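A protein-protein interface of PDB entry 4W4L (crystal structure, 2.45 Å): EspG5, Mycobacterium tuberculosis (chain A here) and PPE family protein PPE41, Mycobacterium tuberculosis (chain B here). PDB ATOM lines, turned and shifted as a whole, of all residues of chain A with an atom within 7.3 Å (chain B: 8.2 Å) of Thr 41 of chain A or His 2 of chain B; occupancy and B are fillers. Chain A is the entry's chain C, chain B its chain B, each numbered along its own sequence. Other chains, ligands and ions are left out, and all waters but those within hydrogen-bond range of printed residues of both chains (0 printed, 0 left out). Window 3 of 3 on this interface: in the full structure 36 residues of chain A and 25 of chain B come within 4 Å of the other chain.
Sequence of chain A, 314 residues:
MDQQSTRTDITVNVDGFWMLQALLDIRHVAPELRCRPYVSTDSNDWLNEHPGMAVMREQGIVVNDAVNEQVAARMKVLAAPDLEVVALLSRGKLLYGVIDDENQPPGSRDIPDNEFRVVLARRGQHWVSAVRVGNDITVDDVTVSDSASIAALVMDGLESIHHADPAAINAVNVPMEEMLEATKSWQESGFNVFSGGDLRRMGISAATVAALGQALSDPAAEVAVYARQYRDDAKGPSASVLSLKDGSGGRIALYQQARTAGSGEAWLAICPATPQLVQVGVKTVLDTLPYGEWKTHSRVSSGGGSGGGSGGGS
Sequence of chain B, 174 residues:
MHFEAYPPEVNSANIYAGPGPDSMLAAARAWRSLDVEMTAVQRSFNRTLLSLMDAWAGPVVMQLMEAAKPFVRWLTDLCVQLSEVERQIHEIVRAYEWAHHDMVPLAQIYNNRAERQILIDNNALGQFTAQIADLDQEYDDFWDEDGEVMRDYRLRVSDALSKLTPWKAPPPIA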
ATOM      1  N   TRP A  18      -3.431  25.320  12.705  1.00  0.00           N
ATOM      2  CA  TRP A  18      -3.983  24.178  13.427  1.00  0.00           C
ATOM      3  C   TRP A  18      -3.799  22.882  12.642  1.00  0.00           C
ATOM      4  O   TRP A  18      -3.575  21.827  13.229  1.00  0.00           O
ATOM      5  CB  TRP A  18      -5.466  24.389  13.735  1.00  0.00           C
ATOM      6  CG  TRP A  18      -6.039  23.303  14.588  1.00  0.00           C
ATOM      7  CD1 TRP A  18      -6.045  23.249  15.951  1.00  0.00           C
ATOM      8  CD2 TRP A  18      -6.681  22.104  14.138  1.00  0.00           C
ATOM      9  NE1 TRP A  18      -6.652  22.095  16.378  1.00  0.00           N
ATOM     10  CE2 TRP A  18      -7.053  21.375  15.285  1.00  0.00           C
ATOM     11  CE3 TRP A  18      -6.978  21.579  12.876  1.00  0.00           C
ATOM     12  CZ2 TRP A  18      -7.708  20.146  15.209  1.00  0.00           C
ATOM     13  CZ3 TRP A  18      -7.630  20.358  12.803  1.00  0.00           C
ATOM     14  CH2 TRP A  18      -7.987  19.656  13.962  1.00  0.00           C
ATOM     15  N   ALA A  22      -1.856  19.593  13.798  1.00  0.00           N
ATOM     16  CA  ALA A  22      -2.464  18.274  13.705  1.00  0.00           C
ATOM     17  C   ALA A  22      -1.572  17.293  12.951  1.00  0.00           C
ATOM     18  O   ALA A  22      -1.389  16.154  13.384  1.00  0.00           O
ATOM     19  CB  ALA A  22      -3.824  18.372  13.037  1.00  0.00           C
ATOM     20  N   ASP A  25       1.510  16.680  15.021  1.00  0.00           N
ATOM     21  CA  ASP A  25       1.135  16.366  16.400  1.00  0.00           C
ATOM     22  C   ASP A  25       1.739  17.348  17.403  1.00  0.00           C
ATOM     23  O   ASP A  25       2.579  16.983  18.228  1.00  0.00           O
ATOM     24  CB  ASP A  25       1.536  14.935  16.767  1.00  0.00           C
ATOM     25  CG  ASP A  25       0.958  14.499  18.102  1.00  0.00           C
ATOM     26  OD1 ASP A  25      -0.272  14.291  18.174  1.00  0.00           O
ATOM     27  OD2 ASP A  25       1.728  14.369  19.077  1.00  0.00           O
ATOM     28  N   ARG A  36      -5.859  27.544  18.620  1.00  0.00           N
ATOM     29  CA  ARG A  36      -6.581  26.565  19.419  1.00  0.00           C
ATOM     30  C   ARG A  36      -5.726  25.316  19.555  1.00  0.00           C
ATOM     31  O   ARG A  36      -4.954  24.994  18.656  1.00  0.00           O
ATOM     32  CB  ARG A  36      -7.959  26.247  18.818  1.00  0.00           C
ATOM     33  CG  ARG A  36      -7.996  26.008  17.328  1.00  0.00           C
ATOM     34  CD  ARG A  36      -9.439  26.019  16.836  1.00  0.00           C
ATOM     35  NE  ARG A  36      -9.541  25.747  15.405  1.00  0.00           N
ATOM     36  CZ  ARG A  36      -9.847  24.559  14.890  1.00  0.00           C
ATOM     37  NH1 ARG A  36     -10.087  23.527  15.688  1.00  0.00           N
ATOM     38  NH2 ARG A  36      -9.916  24.403  13.575  1.00  0.00           N
ATOM     39  N   PRO A  37      -5.838  24.626  20.698  1.00  0.00           N
ATOM     40  CA  PRO A  37      -5.051  23.413  20.940  1.00  0.00           C
ATOM     41  C   PRO A  37      -5.368  22.310  19.944  1.00  0.00           C
ATOM     42  O   PRO A  37      -6.413  22.343  19.296  1.00  0.00           O
ATOM     43  CB  PRO A  37      -5.473  22.991  22.354  1.00  0.00           C
ATOM     44  CG  PRO A  37      -6.035  24.215  22.974  1.00  0.00           C
ATOM     45  CD  PRO A  37      -6.672  24.980  21.857  1.00  0.00           C
ATOM     46  N   TYR A  38      -4.465  21.346  19.824  1.00  0.00           N
ATOM     47  CA  TYR A  38      -4.761  20.134  19.083  1.00  0.00           C
ATOM     48  C   TYR A  38      -4.800  18.941  20.025  1.00  0.00           C
ATOM     49  O   TYR A  38      -3.836  18.665  20.737  1.00  0.00           O
ATOM     50  CB  TYR A  38      -3.736  19.895  17.976  1.00  0.00           C
ATOM     51  CG  TYR A  38      -3.854  18.522  17.351  1.00  0.00           C
ATOM     52  CD1 TYR A  38      -4.992  18.160  16.642  1.00  0.00           C
ATOM     53  CD2 TYR A  38      -2.831  17.587  17.471  1.00  0.00           C
ATOM     54  CE1 TYR A  38      -5.111  16.907  16.069  1.00  0.00           C
ATOM     55  CE2 TYR A  38      -2.940  16.329  16.899  1.00  0.00           C
ATOM     56  CZ  TYR A  38      -4.082  15.997  16.200  1.00  0.00           C
ATOM     57  OH  TYR A  38      -4.205  14.753  15.626  1.00  0.00           O
ATOM     58  N   VAL A  39      -5.928  18.243  20.029  1.00  0.00           N
ATOM     59  CA  VAL A  39      -6.071  17.024  20.809  1.00  0.00           C
ATOM     60  C   VAL A  39      -6.168  15.834  19.864  1.00  0.00           C
ATOM     61  O   VAL A  39      -7.107  15.732  19.077  1.00  0.00           O
ATOM     62  CB  VAL A  39      -7.309  17.080  21.722  1.00  0.00           C
ATOM     63  CG1 VAL A  39      -7.452  15.791  22.509  1.00  0.00           C
ATOM     64  CG2 VAL A  39      -7.219  18.274  22.659  1.00  0.00           C
ATOM     65  N   SER A  40      -5.191  14.936  19.932  1.00  0.00           N
ATOM     66  CA  SER A  40      -5.163  13.803  19.018  1.00  0.00           C
ATOM     67  C   SER A  40      -6.282  12.820  19.333  1.00  0.00           C
ATOM     68  O   SER A  40      -6.406  12.338  20.456  1.00  0.00           O
ATOM     69  CB  SER A  40      -3.809  13.096  19.073  1.00  0.00           C
ATOM     70  OG  SER A  40      -3.560  12.569  20.363  1.00  0.00           O
ATOM     71  N   THR A  41      -7.105  12.541  18.331  1.00  0.00           N
ATOM     72  CA  THR A  41      -8.138  11.526  18.452  1.00  0.00           C
ATOM     73  C   THR A  41      -7.576  10.194  17.968  1.00  0.00           C
ATOM     74  O   THR A  41      -6.367  10.057  17.774  1.00  0.00           O
ATOM     75  CB  THR A  41      -9.400  11.896  17.652  1.00  0.00           C
ATOM     76  OG1 THR A  41      -9.074  12.003  16.261  1.00  0.00           O
ATOM     77  CG2 THR A  41      -9.963  13.222  18.136  1.00  0.00           C
ATOM     78  N   ASP A  42      -8.446   9.206  17.793  1.00  0.00           N
ATOM     79  CA  ASP A  42      -8.020   7.919  17.256  1.00  0.00           C
ATOM     80  C   ASP A  42      -7.847   7.979  15.736  1.00  0.00           C
ATOM     81  O   ASP A  42      -7.335   7.042  15.125  1.00  0.00           O
ATOM     82  CB  ASP A  42      -9.015   6.819  17.641  1.00  0.00           C
ATOM     83  CG  ASP A  42     -10.458   7.211  17.375  1.00  0.00           C
ATOM     84  OD1 ASP A  42     -10.770   8.421  17.419  1.00  0.00           O
ATOM     85  OD2 ASP A  42     -11.283   6.305  17.129  1.00  0.00           O
ATOM     86  N   SER A  43      -8.277   9.082  15.130  1.00  0.00           N
ATOM     87  CA  SER A  43      -8.138   9.261  13.689  1.00  0.00           C
ATOM     88  C   SER A  43      -7.750  10.693  13.339  1.00  0.00           C
ATOM     89  O   SER A  43      -8.384  11.647  13.792  1.00  0.00           O
ATOM     90  CB  SER A  43      -9.436   8.882  12.974  1.00  0.00           C
ATOM     91  OG  SER A  43     -10.521   9.664  13.440  1.00  0.00           O
ATOM     92  N   ASN A  44      -6.700  10.838  12.539  1.00  0.00           N
ATOM     93  CA  ASN A  44      -6.286  12.154  12.068  1.00  0.00           C
ATOM     94  C   ASN A  44      -6.841  12.440  10.676  1.00  0.00           C
ATOM     95  O   ASN A  44      -6.631  13.517  10.121  1.00  0.00           O
ATOM     96  CB  ASN A  44      -4.763  12.271  12.071  1.00  0.00           C
ATOM     97  CG  ASN A  44      -4.289  13.649  12.494  1.00  0.00           C
ATOM     98  OD1 ASN A  44      -5.082  14.482  12.935  1.00  0.00           O
ATOM     99  ND2 ASN A  44      -2.989  13.892  12.371  1.00  0.00           N
ATOM    100  N   ASP A  45      -7.560  11.469  10.124  1.00  0.00           N
ATOM    101  CA  ASP A  45      -8.214  11.629   8.831  1.00  0.00           C
ATOM    102  C   ASP A  45      -9.542  12.356   9.027  1.00  0.00           C
ATOM    103  O   ASP A  45     -10.275  12.615   8.075  1.00  0.00           O
ATOM    104  CB  ASP A  45      -8.430  10.267   8.160  1.00  0.00           C
ATOM    105  CG  ASP A  45      -8.988  10.386   6.751  1.00  0.00           C
ATOM    106  OD1 ASP A  45      -8.660  11.371   6.057  1.00  0.00           O
ATOM    107  OD2 ASP A  45      -9.761   9.494   6.341  1.00  0.00           O
ATOM    108  N   TRP A  46      -9.840  12.684  10.280  1.00  0.00           N
ATOM    109  CA  TRP A  46     -11.089  13.349  10.622  1.00  0.00           C
ATOM    110  C   TRP A  46     -10.985  14.869  10.504  1.00  0.00           C
ATOM    111  O   TRP A  46     -11.981  15.576  10.648  1.00  0.00           O
ATOM    112  CB  TRP A  46     -11.531  12.935  12.027  1.00  0.00           C
ATOM    113  CG  TRP A  46     -12.581  11.852  12.027  1.00  0.00           C
ATOM    114  CD1 TRP A  46     -13.756  11.855  12.722  1.00  0.00           C
ATOM    115  CD2 TRP A  46     -12.562  10.620  11.281  1.00  0.00           C
ATOM    116  NE1 TRP A  46     -14.462  10.704  12.466  1.00  0.00           N
ATOM    117  CE2 TRP A  46     -13.752   9.930  11.585  1.00  0.00           C
ATOM    118  CE3 TRP A  46     -11.651  10.034  10.393  1.00  0.00           C
ATOM    119  CZ2 TRP A  46     -14.056   8.686  11.032  1.00  0.00           C
ATOM    120  CZ3 TRP A  46     -11.956   8.799   9.846  1.00  0.00           C
ATOM    121  CH2 TRP A  46     -13.147   8.139  10.168  1.00  0.00           C
ATOM    122  N   LEU A  47      -9.777  15.370  10.261  1.00  0.00           N
ATOM    123  CA  LEU A  47      -9.608  16.739   9.780  1.00  0.00           C
ATOM    124  C   LEU A  47      -9.566  16.688   8.255  1.00  0.00           C
ATOM    125  O   LEU A  47      -9.609  17.709   7.576  1.00  0.00           O
ATOM    126  CB  LEU A  47      -8.337  17.377  10.347  1.00  0.00           C
ATOM    127  CG  LEU A  47      -7.001  17.010   9.693  1.00  0.00           C
ATOM    128  CD1 LEU A  47      -6.501  18.130   8.794  1.00  0.00           C
ATOM    129  CD2 LEU A  47      -5.960  16.667  10.738  1.00  0.00           C
ATOM    130  N   MET B   1     -16.124  13.724  17.115  1.00  0.00           N
ATOM    131  CA  MET B   1     -15.466  14.830  16.431  1.00  0.00           C
ATOM    132  C   MET B   1     -14.292  15.363  17.241  1.00  0.00           C
ATOM    133  O   MET B   1     -13.724  14.654  18.072  1.00  0.00           O
ATOM    134  CB  MET B   1     -16.462  15.959  16.159  1.00  0.00           C
ATOM    135  CG  MET B   1     -17.142  16.490  17.409  1.00  0.00           C
ATOM    136  SD  MET B   1     -18.039  18.014  17.087  1.00  0.00           S
ATOM    137  CE  MET B   1     -19.046  17.522  15.684  1.00  0.00           C
ATOM    138  N   HIS B   2     -13.930  16.617  16.988  1.00  0.00           N
ATOM    139  CA  HIS B   2     -12.894  17.289  17.767  1.00  0.00           C
ATOM    140  C   HIS B   2     -13.532  18.331  18.675  1.00  0.00           C
ATOM    141  O   HIS B   2     -13.967  19.383  18.212  1.00  0.00           O
ATOM    142  CB  HIS B   2     -11.857  17.951  16.854  1.00  0.00           C
ATOM    143  CG  HIS B   2     -10.862  16.995  16.272  1.00  0.00           C
ATOM    144  ND1 HIS B   2      -9.648  16.730  16.870  1.00  0.00           N
ATOM    145  CD2 HIS B   2     -10.897  16.247  15.144  1.00  0.00           C
ATOM    146  CE1 HIS B   2      -8.980  15.858  16.136  1.00  0.00           C
ATOM    147  NE2 HIS B   2      -9.715  15.548  15.084  1.00  0.00           N
ATOM    148  N   PHE B   3     -13.551  18.060  19.974  1.00  0.00           N
ATOM    149  CA  PHE B   3     -14.236  18.949  20.902  1.00  0.00           C
ATOM    150  C   PHE B   3     -13.356  20.117  21.332  1.00  0.00           C
ATOM    151  O   PHE B   3     -13.837  21.058  21.963  1.00  0.00           O
ATOM    152  CB  PHE B   3     -14.730  18.173  22.123  1.00  0.00           C
ATOM    153  CG  PHE B   3     -15.950  17.336  21.848  1.00  0.00           C
ATOM    154  CD1 PHE B   3     -17.212  17.909  21.847  1.00  0.00           C
ATOM    155  CD2 PHE B   3     -15.834  15.977  21.592  1.00  0.00           C
ATOM    156  CE1 PHE B   3     -18.337  17.144  21.590  1.00  0.00           C
ATOM    157  CE2 PHE B   3     -16.954  15.204  21.337  1.00  0.00           C
ATOM    158  CZ  PHE B   3     -18.207  15.786  21.333  1.00  0.00           C
ATOM    159  N   GLU B   4     -12.077  20.072  20.969  1.00  0.00           N
ATOM    160  CA  GLU B   4     -11.182  21.212  21.184  1.00  0.00           C
ATOM    161  C   GLU B   4     -11.511  22.346  20.214  1.00  0.00           C
ATOM    162  O   GLU B   4     -10.926  23.426  20.284  1.00  0.00           O
ATOM    163  CB  GLU B   4      -9.714  20.807  21.040  1.00  0.00           C
ATOM    164  CG  GLU B   4      -9.300  20.389  19.640  1.00  0.00           C
ATOM    165  CD  GLU B   4      -9.586  18.928  19.345  1.00  0.00           C
ATOM    166  OE1 GLU B   4     -10.461  18.330  20.009  1.00  0.00           O
ATOM    167  OE2 GLU B   4      -8.925  18.373  18.440  1.00  0.00           O
ATOM    168  N   ALA B   5     -12.434  22.095  19.294  1.00  0.00           N
ATOM    169  CA  ALA B   5     -12.989  23.170  18.481  1.00  0.00           C
ATOM    170  C   ALA B   5     -13.719  24.183  19.364  1.00  0.00           C
ATOM    171  O   ALA B   5     -13.982  25.308  18.946  1.00  0.00           O
ATOM    172  CB  ALA B   5     -13.931  22.610  17.425  1.00  0.00           C
ATOM    173  N   TYR B   6     -14.035  23.779  20.591  1.00  0.00           N
ATOM    174  CA  TYR B   6     -14.802  24.620  21.499  1.00  0.00           C
ATOM    175  C   TYR B   6     -13.993  24.971  22.743  1.00  0.00           C
ATOM    176  O   TYR B   6     -13.158  24.185  23.192  1.00  0.00           O
ATOM    177  CB  TYR B   6     -16.106  23.916  21.890  1.00  0.00           C
ATOM    178  CG  TYR B   6     -16.873  23.379  20.705  1.00  0.00           C
ATOM    179  CD1 TYR B   6     -17.081  24.161  19.574  1.00  0.00           C
ATOM    180  CD2 TYR B   6     -17.370  22.082  20.707  1.00  0.00           C
ATOM    181  CE1 TYR B   6     -17.774  23.667  18.485  1.00  0.00           C
ATOM    182  CE2 TYR B   6     -18.064  21.583  19.626  1.00  0.00           C
ATOM    183  CZ  TYR B   6     -18.266  22.380  18.518  1.00  0.00           C
ATOM    184  OH  TYR B   6     -18.955  21.881  17.437  1.00  0.00           O
ATOM    185  N   ASN B  11     -17.375  23.238  26.899  1.00  0.00           N
ATOM    186  CA  ASN B  11     -17.271  21.827  27.269  1.00  0.00           C
ATOM    187  C   ASN B  11     -17.611  21.587  28.744  1.00  0.00           C
ATOM    188  O   ASN B  11     -18.366  20.653  29.088  1.00  0.00           O
ATOM    189  CB  ASN B  11     -15.875  21.300  26.935  1.00  0.00           C
ATOM    190  CG  ASN B  11     -15.670  21.115  25.436  1.00  0.00           C
ATOM    191  OD1 ASN B  11     -16.587  20.710  24.718  1.00  0.00           O
ATOM    192  ND2 ASN B  11     -14.471  21.424  24.956  1.00  0.00           N
ATOM    193  N   TRP B 143      -8.540  24.347  28.073  1.00  0.00           N
ATOM    194  CA  TRP B 143      -9.064  24.043  26.739  1.00  0.00           C
ATOM    195  C   TRP B 143      -8.673  22.632  26.299  1.00  0.00           C
ATOM    196  O   TRP B 143      -9.528  21.789  25.956  1.00  0.00           O
ATOM    197  CB  TRP B 143      -8.540  25.086  25.738  1.00  0.00           C
ATOM    198  CG  TRP B 143      -9.259  25.142  24.420  1.00  0.00           C
ATOM    199  CD1 TRP B 143      -9.721  24.089  23.690  1.00  0.00           C
ATOM    200  CD2 TRP B 143      -9.601  26.322  23.681  1.00  0.00           C
ATOM    201  NE1 TRP B 143     -10.326  24.534  22.543  1.00  0.00           N
ATOM    202  CE2 TRP B 143     -10.267  25.901  22.510  1.00  0.00           C
ATOM    203  CE3 TRP B 143      -9.406  27.692  23.894  1.00  0.00           C
ATOM    204  CZ2 TRP B 143     -10.739  26.801  21.551  1.00  0.00           C
ATOM    205  CZ3 TRP B 143      -9.877  28.584  22.945  1.00  0.00           C
ATOM    206  CH2 TRP B 143     -10.538  28.133  21.788  1.00  0.00           C
ATOM    207  N   GLY B 147     -10.784  19.113  26.108  1.00  0.00           N
ATOM    208  CA  GLY B 147     -10.672  18.385  24.855  1.00  0.00           C
ATOM    209  C   GLY B 147     -10.430  16.896  25.057  1.00  0.00           C
ATOM    210  O   GLY B 147     -11.147  16.061  24.503  1.00  0.00           O
ATOM    211  N   MET B 150     -13.391  15.053  26.756  1.00  0.00           N
ATOM    212  CA  MET B 150     -14.486  14.789  25.827  1.00  0.00           C
ATOM    213  C   MET B 150     -14.102  13.717  24.805  1.00  0.00           C
ATOM    214  O   MET B 150     -14.938  12.900  24.420  1.00  0.00           O
ATOM    215  CB  MET B 150     -14.923  16.069  25.125  1.00  0.00           C
ATOM    216  CG  MET B 150     -15.766  16.985  25.997  1.00  0.00           C
ATOM    217  SD  MET B 150     -17.275  16.193  26.596  1.00  0.00           S
ATOM    218  CE  MET B 150     -18.124  15.826  25.064  1.00  0.00           C
ATOM    219  N   ARG B 151     -12.840  13.703  24.384  1.00  0.00           N
ATOM    220  CA  ARG B 151     -12.352  12.628  23.526  1.00  0.00           C
ATOM    221  C   ARG B 151     -12.580  11.257  24.168  1.00  0.00           C
ATOM    222  O   ARG B 151     -13.194  10.372  23.562  1.00  0.00           O
ATOM    223  CB  ARG B 151     -10.867  12.817  23.216  1.00  0.00           C
ATOM    224  CG  ARG B 151     -10.273  11.719  22.346  1.00  0.00           C
ATOM    225  CD  ARG B 151      -8.766  11.678  22.497  1.00  0.00           C
ATOM    226  NE  ARG B 151      -8.392  11.597  23.906  1.00  0.00           N
ATOM    227  CZ  ARG B 151      -7.235  12.024  24.404  1.00  0.00           C
ATOM    228  NH1 ARG B 151      -6.324  12.570  23.609  1.00  0.00           N
ATOM    229  NH2 ARG B 151      -6.993  11.911  25.702  1.00  0.00           N
ATOM    230  N   ASP B 152     -12.100  11.093  25.401  1.00  0.00           N
ATOM    231  CA  ASP B 152     -12.220   9.807  26.096  1.00  0.00           C
ATOM    232  C   ASP B 152     -13.680   9.426  26.354  1.00  0.00           C
ATOM    233  O   ASP B 152     -14.059   8.252  26.243  1.00  0.00           O
ATOM    234  CB  ASP B 152     -11.444   9.839  27.414  1.00  0.00           C
ATOM    235  CG  ASP B 152      -9.962  10.099  27.207  1.00  0.00           C
ATOM    236  OD1 ASP B 152      -9.451   9.807  26.104  1.00  0.00           O
ATOM    237  OD2 ASP B 152      -9.308  10.598  28.146  1.00  0.00           O
ATOM    238  N   ARG B 154     -16.254  10.320  24.496  1.00  0.00           N
ATOM    239  CA  ARG B 154     -16.767   9.892  23.207  1.00  0.00           C
ATOM    240  C   ARG B 154     -16.342   8.466  22.905  1.00  0.00           C
ATOM    241  O   ARG B 154     -17.163   7.650  22.513  1.00  0.00           O
ATOM    242  CB  ARG B 154     -16.292  10.816  22.082  1.00  0.00           C
ATOM    243  CG  ARG B 154     -16.791  10.376  20.717  1.00  0.00           C
ATOM    244  CD  ARG B 154     -16.192  11.196  19.589  1.00  0.00           C
ATOM    245  NE  ARG B 154     -14.757  10.971  19.434  1.00  0.00           N
ATOM    246  CZ  ARG B 154     -14.220   9.865  18.924  1.00  0.00           C
ATOM    247  NH1 ARG B 154     -14.997   8.862  18.530  1.00  0.00           N
ATOM    248  NH2 ARG B 154     -12.902   9.756  18.819  1.00  0.00           N
ATOM    249  N   LEU B 155     -15.057   8.177  23.083  1.00  0.00           N
ATOM    250  CA  LEU B 155     -14.536   6.849  22.792  1.00  0.00           C
ATOM    251  C   LEU B 155     -15.214   5.767  23.625  1.00  0.00           C
ATOM    252  O   LEU B 155     -15.607   4.733  23.087  1.00  0.00           O
ATOM    253  CB  LEU B 155     -13.026   6.812  23.011  1.00  0.00           C
ATOM    254  CG  LEU B 155     -12.255   7.528  21.907  1.00  0.00           C
ATOM    255  CD1 LEU B 155     -10.834   7.800  22.347  1.00  0.00           C
ATOM    256  CD2 LEU B 155     -12.292   6.704  20.622  1.00  0.00           C
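Hydrophobic or aromatic side chains of chain A that line the printed part of chain B: Trp 18, Pro 37 and Val 39.
Printed residues of chain B that touch a printed residue of chain A: His 2, Glu 4, Trp 143, Arg 151, Arg 154 and Leu 155.
Hydrophobic or aromatic side chains of chain B within 4 Å of the printed part of chain A: His 2, Trp 143 and Leu 155.
Among the printed residues, 11 pairs touch across the chains.
Among the printed residues, Asp or Glu carboxylates within 4 Å of a Lys or Arg side-chain nitrogen of the other chain: Asp 42 of chain A with Arg 154 of chain B.
The side-chain carboxylate (OE2) of Glu 4 of chain B sits at hydrogen-bond distance from the backbone NH (N) of Val 39 of chain A (3.4 Å).
NH1 of Arg 151 of chain B sits at hydrogen-bond distance from O of Ser 40 of chain A, at 3.2 Å.
The guanidinium group (NH2) of Arg 154 of chain B is in salt-bridge range of the side-chain carboxylate (OD1) of Asp 42 of chain A (2.9 Å).
Among the printed residues, merely in contact across the chains: Trp 18 of chain A with Glu 4 of chain B (3.9 Å), Arg 36 of chain A with Trp 143 of chain B (3.9 Å), Pro 37 of chain A with Glu 4 of chain B (3.5 Å), Pro 37 of chain A with Trp 143 of chain B (3.6 Å), Val 39 of chain A with His 2 of chain B (3.5 Å), Val 39 of chain A with Arg 151 of chain B (3.6 Å), Thr 41 of chain A with His 2 of chain B (3.5 Å) and Asp 42 of chain A with Leu 155 of chain B (3.7 Å).
Ser 40 of chain A touches just one residue of chain B: Arg 151.
Printed residues of chain B within 4 Å of Thr 41 of chain A: His 2.
Trp 46 of chain A touches none of the printed residues of chain B.
Of the printed residues of chain A, His 2 of chain B touches Val 39 (3.5 Å) and Thr 41 (3.5 Å).
Of the printed residues of chain A, Arg 151 of chain B touches Val 39 and Ser 40.
Printed residues of chain A within 4 Å of Arg 154 of chain B: Asp 42 (2.9 Å).
Of the printed residues of chain A, Leu 155 of chain B touches Asp 42.
The nearest printed residue of chain B that does not touch Thr 41 of chain A is Met 1 of chain B (4.02 Å).
The nearest printed residue of chain A that does not touch His 2 of chain B is Tyr 38 of chain A (4.01 Å).
The indole nitrogen (NE1) of Trp 143 of chain B lies within hydrogen-bond range of the backbone carbonyl oxygen (O) of Glu 4 of chain B (2.6 Å).
The indole nitrogen of Trp 143 of chain B sits at hydrogen-bond distance from the backbone carbonyl oxygen of Tyr 6 of chain B (2.9 Å).
The guanidinium group (NE) of Arg 151 of chain B is in salt-bridge range of the side-chain carboxylate (OD1) of Asp 152 of chain B (3.0 Å).
O of Pro 37 of chain A lies within hydrogen-bond range of NE1 of Trp 18 of chain A.
OG1 of Thr 41 of chain A sits at hydrogen-bond distance from O of Ser 43 of chain A.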
